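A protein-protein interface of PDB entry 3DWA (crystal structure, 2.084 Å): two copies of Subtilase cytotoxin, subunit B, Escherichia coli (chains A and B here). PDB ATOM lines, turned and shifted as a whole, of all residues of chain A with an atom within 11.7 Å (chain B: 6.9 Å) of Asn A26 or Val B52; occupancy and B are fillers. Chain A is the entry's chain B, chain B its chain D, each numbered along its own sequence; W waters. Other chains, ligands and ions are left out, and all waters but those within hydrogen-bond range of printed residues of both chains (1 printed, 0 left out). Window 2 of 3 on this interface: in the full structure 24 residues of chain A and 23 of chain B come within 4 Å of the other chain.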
ATOM      1  N   GLY A  22     -10.635   0.799  24.074  1.00  0.00           N
ATOM      2  CA  GLY A  22     -10.449   2.212  23.929  1.00  0.00           C
ATOM      3  C   GLY A  22      -9.051   2.526  23.452  1.00  0.00           C
ATOM      4  O   GLY A  22      -8.417   1.685  22.830  1.00  0.00           O
ATOM      5  N   GLN A  23      -8.604   3.765  23.686  1.00  0.00           N
ATOM      6  CA  GLN A  23      -7.293   4.223  23.218  1.00  0.00           C
ATOM      7  C   GLN A  23      -6.692   5.093  24.319  1.00  0.00           C
ATOM      8  O   GLN A  23      -7.428   5.830  24.971  1.00  0.00           O
ATOM      9  CB  GLN A  23      -7.449   5.080  21.956  1.00  0.00           C
ATOM     10  CG  GLN A  23      -6.121   5.611  21.412  1.00  0.00           C
ATOM     11  CD  GLN A  23      -6.242   6.436  20.128  1.00  0.00           C
ATOM     12  OE1 GLN A  23      -6.834   5.978  19.110  1.00  0.00           O
ATOM     13  NE2 GLN A  23      -5.680   7.667  20.153  1.00  0.00           N
ATOM     14  N   ILE A  24      -5.368   5.041  24.500  1.00  0.00           N
ATOM     15  CA  ILE A  24      -4.661   5.980  25.379  1.00  0.00           C
ATOM     16  C   ILE A  24      -3.289   6.301  24.713  1.00  0.00           C
ATOM     17  O   ILE A  24      -2.618   5.418  24.204  1.00  0.00           O
ATOM     18  CB  ILE A  24      -4.578   5.478  26.865  1.00  0.00           C
ATOM     19  CG1 ILE A  24      -3.967   6.570  27.779  1.00  0.00           C
ATOM     20  CG2 ILE A  24      -3.785   4.182  26.972  1.00  0.00           C
ATOM     21  CD1 ILE A  24      -3.962   6.237  29.304  1.00  0.00           C
ATOM     22  N   ASP A  25      -2.923   7.585  24.625  1.00  0.00           N
ATOM     23  CA  ASP A  25      -1.620   7.962  24.083  1.00  0.00           C
ATOM     24  C   ASP A  25      -1.331   7.296  22.764  1.00  0.00           C
ATOM     25  O   ASP A  25      -0.304   6.617  22.580  1.00  0.00           O
ATOM     26  CB  ASP A  25      -0.495   7.608  25.076  1.00  0.00           C
ATOM     27  CG  ASP A  25      -0.540   8.465  26.305  1.00  0.00           C
ATOM     28  OD1 ASP A  25      -1.113   9.573  26.230  1.00  0.00           O
ATOM     29  OD2 ASP A  25      -0.041   8.027  27.364  1.00  0.00           O
ATOM     30  N   ASN A  26      -2.245   7.503  21.835  1.00  0.00           N
ATOM     31  CA  ASN A  26      -2.082   7.006  20.480  1.00  0.00           C
ATOM     32  C   ASN A  26      -2.026   5.473  20.335  1.00  0.00           C
ATOM     33  O   ASN A  26      -1.655   4.976  19.275  1.00  0.00           O
ATOM     34  CB  ASN A  26      -0.854   7.669  19.835  1.00  0.00           C
ATOM     35  CG  ASN A  26      -1.007   7.834  18.330  1.00  0.00           C
ATOM     36  OD1 ASN A  26      -0.131   7.434  17.570  1.00  0.00           O
ATOM     37  ND2 ASN A  26      -2.138   8.418  17.888  1.00  0.00           N
ATOM     38  N   LYS A  27      -2.416   4.737  21.387  1.00  0.00           N
ATOM     39  CA  LYS A  27      -2.444   3.256  21.362  1.00  0.00           C
ATOM     40  C   LYS A  27      -3.812   2.632  21.699  1.00  0.00           C
ATOM     41  O   LYS A  27      -4.336   2.868  22.802  1.00  0.00           O
ATOM     42  CB  LYS A  27      -1.419   2.681  22.350  1.00  0.00           C
ATOM     43  CG  LYS A  27       0.009   3.039  22.077  1.00  0.00           C
ATOM     44  CD  LYS A  27       0.893   2.620  23.255  1.00  0.00           C
ATOM     45  CE  LYS A  27       2.267   3.280  23.217  1.00  0.00           C
ATOM     46  NZ  LYS A  27       3.083   2.818  22.056  1.00  0.00           N
ATOM     47  N   PRO A  28      -4.359   1.773  20.792  1.00  0.00           N
ATOM     48  CA  PRO A  28      -5.567   1.061  21.150  1.00  0.00           C
ATOM     49  C   PRO A  28      -5.262   0.060  22.284  1.00  0.00           C
ATOM     50  O   PRO A  28      -4.161  -0.447  22.386  1.00  0.00           O
ATOM     51  CB  PRO A  28      -5.958   0.298  19.839  1.00  0.00           C
ATOM     52  CG  PRO A  28      -4.685   0.092  19.134  1.00  0.00           C
ATOM     53  CD  PRO A  28      -3.880   1.381  19.446  1.00  0.00           C
ATOM     54  N   TYR A  29      -6.223  -0.213  23.145  1.00  0.00           N
ATOM     55  CA  TYR A  29      -6.006  -1.277  24.139  1.00  0.00           C
ATOM     56  C   TYR A  29      -7.388  -1.971  24.311  1.00  0.00           C
ATOM     57  O   TYR A  29      -8.386  -1.362  23.944  1.00  0.00           O
ATOM     58  CB  TYR A  29      -5.546  -0.623  25.488  1.00  0.00           C
ATOM     59  CG  TYR A  29      -6.625   0.240  26.137  1.00  0.00           C
ATOM     60  CD1 TYR A  29      -7.584  -0.320  26.972  1.00  0.00           C
ATOM     61  CD2 TYR A  29      -6.685   1.615  25.884  1.00  0.00           C
ATOM     62  CE1 TYR A  29      -8.608   0.468  27.541  1.00  0.00           C
ATOM     63  CE2 TYR A  29      -7.670   2.406  26.460  1.00  0.00           C
ATOM     64  CZ  TYR A  29      -8.625   1.835  27.266  1.00  0.00           C
ATOM     65  OH  TYR A  29      -9.601   2.628  27.778  1.00  0.00           O
ATOM     66  N   PHE A  30      -7.459  -3.168  24.898  1.00  0.00           N
ATOM     67  CA  PHE A  30      -8.736  -3.700  25.373  1.00  0.00           C
ATOM     68  C   PHE A  30      -8.560  -4.157  26.809  1.00  0.00           C
ATOM     69  O   PHE A  30      -7.432  -4.405  27.269  1.00  0.00           O
ATOM     70  CB  PHE A  30      -9.278  -4.866  24.508  1.00  0.00           C
ATOM     71  CG  PHE A  30      -8.467  -6.112  24.609  1.00  0.00           C
ATOM     72  CD1 PHE A  30      -8.893  -7.188  25.397  1.00  0.00           C
ATOM     73  CD2 PHE A  30      -7.244  -6.213  23.913  1.00  0.00           C
ATOM     74  CE1 PHE A  30      -8.110  -8.322  25.489  1.00  0.00           C
ATOM     75  CE2 PHE A  30      -6.473  -7.333  23.980  1.00  0.00           C
ATOM     76  CZ  PHE A  30      -6.894  -8.410  24.795  1.00  0.00           C
ATOM     77  N   SER A  46      -4.628  -5.356  27.654  1.00  0.00           N
ATOM     78  CA  SER A  46      -3.537  -5.466  26.721  1.00  0.00           C
ATOM     79  C   SER A  46      -3.540  -4.205  25.861  1.00  0.00           C
ATOM     80  O   SER A  46      -4.606  -3.701  25.492  1.00  0.00           O
ATOM     81  CB  SER A  46      -3.698  -6.757  25.864  1.00  0.00           C
ATOM     82  OG  SER A  46      -2.649  -6.849  24.913  1.00  0.00           O
ATOM     83  N   MET A  47      -2.361  -3.672  25.551  1.00  0.00           N
ATOM     84  CA  MET A  47      -2.269  -2.423  24.816  1.00  0.00           C
ATOM     85  C   MET A  47      -1.329  -2.570  23.645  1.00  0.00           C
ATOM     86  O   MET A  47      -0.247  -3.115  23.804  1.00  0.00           O
ATOM     87  CB  MET A  47      -1.733  -1.314  25.736  1.00  0.00           C
ATOM     88  CG  MET A  47      -1.687   0.072  25.043  1.00  0.00           C
ATOM     89  SD  MET A  47      -1.062   1.405  26.360  1.00  0.00           S
ATOM     90  CE  MET A  47      -2.225   0.951  27.843  1.00  0.00           C
ATOM     91  N   LYS A  48      -1.741  -2.087  22.474  1.00  0.00           N
ATOM     92  CA  LYS A  48      -0.928  -2.276  21.263  1.00  0.00           C
ATOM     93  C   LYS A  48       0.340  -1.436  21.386  1.00  0.00           C
ATOM     94  O   LYS A  48       0.298  -0.311  21.929  1.00  0.00           O
ATOM     95  CB  LYS A  48      -1.701  -1.865  20.008  1.00  0.00           C
ATOM     96  CG  LYS A  48      -0.875  -1.957  18.680  1.00  0.00           C
ATOM     97  CD  LYS A  48      -1.646  -1.351  17.503  1.00  0.00           C
ATOM     98  CE  LYS A  48      -1.115  -1.775  16.162  1.00  0.00           C
ATOM     99  NZ  LYS A  48      -2.098  -1.269  15.102  1.00  0.00           N
ATOM    100  N   ASN A  49       1.465  -2.005  20.963  1.00  0.00           N
ATOM    101  CA  ASN A  49       2.767  -1.334  21.048  1.00  0.00           C
ATOM    102  C   ASN A  49       3.172  -0.948  22.474  1.00  0.00           C
ATOM    103  O   ASN A  49       4.047  -0.104  22.610  1.00  0.00           O
ATOM    104  CB  ASN A  49       2.777   0.001  20.258  1.00  0.00           C
ATOM    105  CG  ASN A  49       2.477  -0.156  18.782  1.00  0.00           C
ATOM    106  OD1 ASN A  49       1.666   0.606  18.216  1.00  0.00           O
ATOM    107  ND2 ASN A  49       3.166  -1.089  18.127  1.00  0.00           N
ATOM    108  N   SER A  50       2.527  -1.481  23.519  1.00  0.00           N
ATOM    109  CA  SER A  50       2.960  -1.180  24.892  1.00  0.00           C
ATOM    110  C   SER A  50       4.362  -1.743  25.116  1.00  0.00           C
ATOM    111  O   SER A  50       4.824  -2.591  24.356  1.00  0.00           O
ATOM    112  CB  SER A  50       1.986  -1.710  25.943  1.00  0.00           C
ATOM    113  OG  SER A  50       1.869  -3.125  25.927  1.00  0.00           O
ATOM    114  N   SER A  51       5.057  -1.274  26.151  1.00  0.00           N
ATOM    115  CA  SER A  51       6.500  -1.513  26.203  1.00  0.00           C
ATOM    116  C   SER A  51       6.896  -2.963  26.327  1.00  0.00           C
ATOM    117  O   SER A  51       7.702  -3.426  25.552  1.00  0.00           O
ATOM    118  CB  SER A  51       7.192  -0.686  27.292  1.00  0.00           C
ATOM    119  OG  SER A  51       8.545  -1.115  27.415  1.00  0.00           O
ATOM    120  N   GLY A  54       3.354  -5.663  24.523  1.00  0.00           N
ATOM    121  CA  GLY A  54       2.558  -5.210  23.402  1.00  0.00           C
ATOM    122  C   GLY A  54       2.689  -6.028  22.134  1.00  0.00           C
ATOM    123  O   GLY A  54       1.783  -5.987  21.282  1.00  0.00           O
ATOM    124  N   PHE A  57      -0.477  -8.057  21.747  1.00  0.00           N
ATOM    125  CA  PHE A  57      -1.807  -7.425  21.641  1.00  0.00           C
ATOM    126  C   PHE A  57      -2.780  -8.084  20.637  1.00  0.00           C
ATOM    127  O   PHE A  57      -3.920  -8.406  20.989  1.00  0.00           O
ATOM    128  CB  PHE A  57      -1.673  -5.918  21.356  1.00  0.00           C
ATOM    129  CG  PHE A  57      -3.013  -5.231  21.062  1.00  0.00           C
ATOM    130  CD1 PHE A  57      -3.846  -4.834  22.090  1.00  0.00           C
ATOM    131  CD2 PHE A  57      -3.393  -4.940  19.751  1.00  0.00           C
ATOM    132  CE1 PHE A  57      -5.096  -4.157  21.805  1.00  0.00           C
ATOM    133  CE2 PHE A  57      -4.597  -4.296  19.460  1.00  0.00           C
ATOM    134  CZ  PHE A  57      -5.459  -3.900  20.502  1.00  0.00           C
ATOM    135  N   TRP A  83       0.330  -0.922  34.079  1.00  0.00           N
ATOM    136  CA  TRP A  83      -0.333   0.345  33.677  1.00  0.00           C
ATOM    137  C   TRP A  83      -0.221   1.318  34.859  1.00  0.00           C
ATOM    138  O   TRP A  83      -0.423   0.931  36.001  1.00  0.00           O
ATOM    139  CB  TRP A  83      -1.811   0.126  33.256  1.00  0.00           C
ATOM    140  CG  TRP A  83      -1.939  -1.126  32.307  1.00  0.00           C
ATOM    141  CD1 TRP A  83      -2.700  -2.234  32.498  1.00  0.00           C
ATOM    142  CD2 TRP A  83      -1.156  -1.378  31.139  1.00  0.00           C
ATOM    143  NE1 TRP A  83      -2.486  -3.149  31.472  1.00  0.00           N
ATOM    144  CE2 TRP A  83      -1.545  -2.633  30.630  1.00  0.00           C
ATOM    145  CE3 TRP A  83      -0.186  -0.639  30.444  1.00  0.00           C
ATOM    146  CZ2 TRP A  83      -0.996  -3.164  29.479  1.00  0.00           C
ATOM    147  CZ3 TRP A  83       0.341  -1.170  29.300  1.00  0.00           C
ATOM    148  CH2 TRP A  83      -0.058  -2.420  28.835  1.00  0.00           C
ATOM    149  N   TYR A  85      -0.942   5.174  34.492  1.00  0.00           N
ATOM    150  CA  TYR A  85      -1.751   6.414  34.426  1.00  0.00           C
ATOM    151  C   TYR A  85      -2.825   6.298  35.503  1.00  0.00           C
ATOM    152  O   TYR A  85      -3.715   5.431  35.399  1.00  0.00           O
ATOM    153  CB  TYR A  85      -2.315   6.680  33.008  1.00  0.00           C
ATOM    154  CG  TYR A  85      -3.054   7.993  32.891  1.00  0.00           C
ATOM    155  CD1 TYR A  85      -2.410   9.194  33.193  1.00  0.00           C
ATOM    156  CD2 TYR A  85      -4.396   8.039  32.489  1.00  0.00           C
ATOM    157  CE1 TYR A  85      -3.090  10.399  33.138  1.00  0.00           C
ATOM    158  CE2 TYR A  85      -5.071   9.228  32.417  1.00  0.00           C
ATOM    159  CZ  TYR A  85      -4.413  10.416  32.741  1.00  0.00           C
ATOM    160  OH  TYR A  85      -5.066  11.627  32.692  1.00  0.00           O
ATOM    161  N   PHE A  88      -6.611   5.775  34.675  1.00  0.00           N
ATOM    162  CA  PHE A  88      -6.700   4.466  33.991  1.00  0.00           C
ATOM    163  C   PHE A  88      -6.715   3.311  34.994  1.00  0.00           C
ATOM    164  O   PHE A  88      -7.634   2.444  34.979  1.00  0.00           O
ATOM    165  CB  PHE A  88      -5.542   4.335  32.963  1.00  0.00           C
ATOM    166  CG  PHE A  88      -5.579   3.056  32.120  1.00  0.00           C
ATOM    167  CD1 PHE A  88      -5.970   3.104  30.784  1.00  0.00           C
ATOM    168  CD2 PHE A  88      -5.154   1.824  32.658  1.00  0.00           C
ATOM    169  CE1 PHE A  88      -5.965   1.914  29.964  1.00  0.00           C
ATOM    170  CE2 PHE A  88      -5.136   0.659  31.903  1.00  0.00           C
ATOM    171  CZ  PHE A  88      -5.551   0.687  30.534  1.00  0.00           C
ATOM    172  N   GLU B   1      -4.048  11.730  25.623  1.00  0.00           N
ATOM    173  CA  GLU B   1      -5.533  11.649  25.572  1.00  0.00           C
ATOM    174  C   GLU B   1      -5.935  10.210  25.935  1.00  0.00           C
ATOM    175  O   GLU B   1      -5.106   9.280  25.879  1.00  0.00           O
ATOM    176  CB  GLU B   1      -6.005  12.025  24.153  1.00  0.00           C
ATOM    177  CG  GLU B   1      -5.918  10.870  23.068  1.00  0.00           C
ATOM    178  CD  GLU B   1      -4.536  10.298  22.800  1.00  0.00           C
ATOM    179  OE1 GLU B   1      -4.469   9.214  22.182  1.00  0.00           O
ATOM    180  OE2 GLU B   1      -3.506  10.895  23.211  1.00  0.00           O
ATOM    181  N   SER B  50      -6.799   9.124  10.862  1.00  0.00           N
ATOM    182  CA  SER B  50      -7.269  10.493  10.939  1.00  0.00           C
ATOM    183  C   SER B  50      -7.790  10.802  12.290  1.00  0.00           C
ATOM    184  O   SER B  50      -8.556  10.014  12.873  1.00  0.00           O
ATOM    185  CB  SER B  50      -8.361  10.857   9.911  1.00  0.00           C
ATOM    186  OG  SER B  50      -8.449   9.923   8.840  1.00  0.00           O
ATOM    187  N   SER B  51      -7.394  12.006  12.731  1.00  0.00           N
ATOM    188  CA  SER B  51      -7.563  12.563  14.085  1.00  0.00           C
ATOM    189  C   SER B  51      -6.558  11.917  15.042  1.00  0.00           C
ATOM    190  O   SER B  51      -5.773  11.074  14.631  1.00  0.00           O
ATOM    191  CB  SER B  51      -9.010  12.481  14.612  1.00  0.00           C
ATOM    192  OG  SER B  51      -9.371  11.160  15.032  1.00  0.00           O
ATOM    193  N   VAL B  52      -6.582  12.335  16.300  1.00  0.00           N
ATOM    194  CA  VAL B  52      -5.816  11.699  17.352  1.00  0.00           C
ATOM    195  C   VAL B  52      -6.336  10.256  17.600  1.00  0.00           C
ATOM    196  O   VAL B  52      -5.577   9.387  18.046  1.00  0.00           O
ATOM    197  CB  VAL B  52      -5.804  12.582  18.659  1.00  0.00           C
ATOM    198  CG1 VAL B  52      -5.446  14.083  18.293  1.00  0.00           C
ATOM    199  CG2 VAL B  52      -7.123  12.532  19.398  1.00  0.00           C
ATOM    200  N   TRP B  53      -7.598  10.006  17.222  1.00  0.00           N
ATOM    201  CA  TRP B  53      -8.234   8.704  17.392  1.00  0.00           C
ATOM    202  C   TRP B  53      -8.046   7.705  16.262  1.00  0.00           C
ATOM    203  O   TRP B  53      -8.566   6.586  16.319  1.00  0.00           O
ATOM    204  CB  TRP B  53      -9.708   8.879  17.711  1.00  0.00           C
ATOM    205  CG  TRP B  53      -9.945   9.865  18.794  1.00  0.00           C
ATOM    206  CD1 TRP B  53     -10.402  11.148  18.657  1.00  0.00           C
ATOM    207  CD2 TRP B  53      -9.760   9.651  20.213  1.00  0.00           C
ATOM    208  NE1 TRP B  53     -10.503  11.741  19.906  1.00  0.00           N
ATOM    209  CE2 TRP B  53     -10.133  10.841  20.869  1.00  0.00           C
ATOM    210  CE3 TRP B  53      -9.326   8.556  20.982  1.00  0.00           C
ATOM    211  CZ2 TRP B  53     -10.084  10.980  22.272  1.00  0.00           C
ATOM    212  CZ3 TRP B  53      -9.238   8.697  22.363  1.00  0.00           C
ATOM    213  CH2 TRP B  53      -9.630   9.895  22.997  1.00  0.00           C
ATOM    214  N   GLY B  54      -7.307   8.103  15.239  1.00  0.00           N
ATOM    215  CA  GLY B  54      -7.001   7.236  14.097  1.00  0.00           C
ATOM    216  C   GLY B  54      -6.382   5.874  14.402  1.00  0.00           C
ATOM    217  O   GLY B  54      -6.631   4.893  13.675  1.00  0.00           O
ATOM    218  N   ALA B  55      -5.612   5.804  15.497  1.00  0.00           N
ATOM    219  CA  ALA B  55      -4.878   4.623  15.897  1.00  0.00           C
ATOM    220  C   ALA B  55      -5.778   3.486  16.305  1.00  0.00           C
ATOM    221  O   ALA B  55      -5.351   2.349  16.288  1.00  0.00           O
ATOM    222  CB  ALA B  55      -3.915   4.967  17.094  1.00  0.00           C
ATOM    223  N   SER B  56      -6.998   3.801  16.711  1.00  0.00           N
ATOM    224  CA  SER B  56      -7.988   2.825  17.171  1.00  0.00           C
ATOM    225  C   SER B  56      -8.885   2.250  16.056  1.00  0.00           C
ATOM    226  O   SER B  56      -9.719   1.385  16.326  1.00  0.00           O
ATOM    227  CB  SER B  56      -8.930   3.531  18.151  1.00  0.00           C
ATOM    228  OG  SER B  56      -8.304   3.750  19.387  1.00  0.00           O
ATOM    229  N   GLU B  79     -16.372  11.531  20.897  1.00  0.00           N
ATOM    230  CA  GLU B  79     -15.894  12.888  21.053  1.00  0.00           C
ATOM    231  C   GLU B  79     -16.545  13.800  19.979  1.00  0.00           C
ATOM    232  O   GLU B  79     -16.245  13.671  18.811  1.00  0.00           O
ATOM    233  CB  GLU B  79     -14.362  12.959  21.005  1.00  0.00           C
ATOM    234  CG  GLU B  79     -13.802  14.401  21.113  1.00  0.00           C
ATOM    235  CD  GLU B  79     -12.343  14.452  21.577  1.00  0.00           C
ATOM    236  OE1 GLU B  79     -12.077  14.338  22.829  1.00  0.00           O
ATOM    237  OE2 GLU B  79     -11.451  14.589  20.697  1.00  0.00           O
ATOM    238  N   VAL B  82     -15.119  16.495  16.088  1.00  0.00           N
ATOM    239  CA  VAL B  82     -13.900  16.038  15.435  1.00  0.00           C
ATOM    240  C   VAL B  82     -13.938  16.095  13.901  1.00  0.00           C
ATOM    241  O   VAL B  82     -12.937  16.490  13.272  1.00  0.00           O
ATOM    242  CB  VAL B  82     -13.522  14.631  15.921  1.00  0.00           C
ATOM    243  CG1 VAL B  82     -12.345  14.071  15.121  1.00  0.00           C
ATOM    244  CG2 VAL B  82     -13.228  14.643  17.440  1.00  0.00           C
ATOM    245  N   TRP B  83     -15.045  15.651  13.282  1.00  0.00           N
ATOM    246  CA  TRP B  83     -15.124  15.672  11.804  1.00  0.00           C
ATOM    247  C   TRP B  83     -15.699  17.053  11.443  1.00  0.00           C
ATOM    248  O   TRP B  83     -16.643  17.497  12.083  1.00  0.00           O
ATOM    249  CB  TRP B  83     -15.925  14.462  11.227  1.00  0.00           C
ATOM    250  CG  TRP B  83     -15.509  13.159  11.906  1.00  0.00           C
ATOM    251  CD1 TRP B  83     -16.297  12.340  12.664  1.00  0.00           C
ATOM    252  CD2 TRP B  83     -14.173  12.616  11.986  1.00  0.00           C
ATOM    253  NE1 TRP B  83     -15.544  11.289  13.171  1.00  0.00           N
ATOM    254  CE2 TRP B  83     -14.242  11.442  12.781  1.00  0.00           C
ATOM    255  CE3 TRP B  83     -12.932  12.988  11.435  1.00  0.00           C
ATOM    256  CZ2 TRP B  83     -13.116  10.671  13.071  1.00  0.00           C
ATOM    257  CZ3 TRP B  83     -11.816  12.202  11.706  1.00  0.00           C
ATOM    258  CH2 TRP B  83     -11.919  11.052  12.513  1.00  0.00           C
HETATM  259  O   HOH W   1      -2.986   1.592  15.647  1.00  0.00           O
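Among the printed residues, merely in contact across the chains: Asn A26 with Ala B55 (3.1 Å), Ile A24 with Glu B1 (3.4 Å), Asn A26 with Val B52 (3.6 Å), Pro A28 with Ala B55 (3.6 Å) and Gln A23 with Ala B55 (3.7 Å).
Of the printed residues of chain B, Gln A23 touches Glu B1 (2.8 Å), Val B52 (2.7 Å), Trp B53 (3.3 Å), Ala B55 (3.7 Å) and Ser B56 (2.7 Å).
Printed residues of chain B within 4 Å of Ile A24: Glu B1.
Of chain B, only Glu B1 (2.8 Å), Val B52 (3.6 Å) and Ala B55 (3.1 Å) come within 4 Å of Asn A26.
Printed residues of chain B within 4 Å of Pro A28: Ala B55 (3.6 Å).
No residue of chain A comes within 4 Å of Ser B51.
Val B52 touches just these residues of chain A: Gln A23 (2.7 Å) and Asn A26 (3.6 Å).
No residue of chain A comes within 4 Å of Gly B54.
Of chain A, only Gln A23, Asn A26 and Pro A28 come within 4 Å of Ala B55.
Printed residues of chain A within 4 Å of Ser B56: Gln A23 (2.7 Å).
The nearest residue of chain B that does not touch Asn A26 is Ser B51 (5.6 Å).
The nearest residue of chain A that does not touch Val B52 is Lys A27 (6.5 Å).
Water W1 lies within hydrogen-bond range of the backbone carbonyl oxygen of Ala B55 (2.6 Å) and the side-chain amino group of Lys A48 (3.0 Å).
NE2 of Gln A23 lies within hydrogen-bond range of OE1 of Glu B1 (2.8 Å).
The backbone carbonyl oxygen of Val B52 lies within hydrogen-bond range of the side-chain amide nitrogen of Gln A23 (2.7 Å).
The backbone carbonyl oxygen (O) of Trp B53 lies close to the side-chain amide oxygen (OE1) of Gln A23 (3.3 Å).
The side-chain amide oxygen (OE1) of Gln A23 is in hydrogen-bond range of the side-chain hydroxyl (OG) of Ser B56, at 2.7 Å.
The backbone carbonyl oxygen of Glu B1 lies within hydrogen-bond range of the backbone NH of Asp A25 (3.0 Å).
The backbone NH (N) of Asn A26 sits at hydrogen-bond distance from the side-chain carboxylate (OE1) of Glu B1 (2.8 Å).
Of the 11 printed residues of chain B, 5 touch a printed residue of chain A.
Among the printed residues, no Asp or Glu carboxylate lies within 4 Å of a Lys or Arg side-chain nitrogen of the other chain.
4 positions are printed for both chains.
Of the 11 pairs that touch across the chains among the printed residues, none has its exchanged pair printed and touching as well.
N of Lys A48 is in hydrogen-bond range of O of Pro A28, 2.9 Å away.
The side-chain hydroxyl (OG) of Ser B51 is in hydrogen-bond range of the backbone NH (N) of Trp B53 (3.0 Å).
The side-chain carboxylate of Glu B79 lies within hydrogen-bond range of the indole nitrogen of Trp B53.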
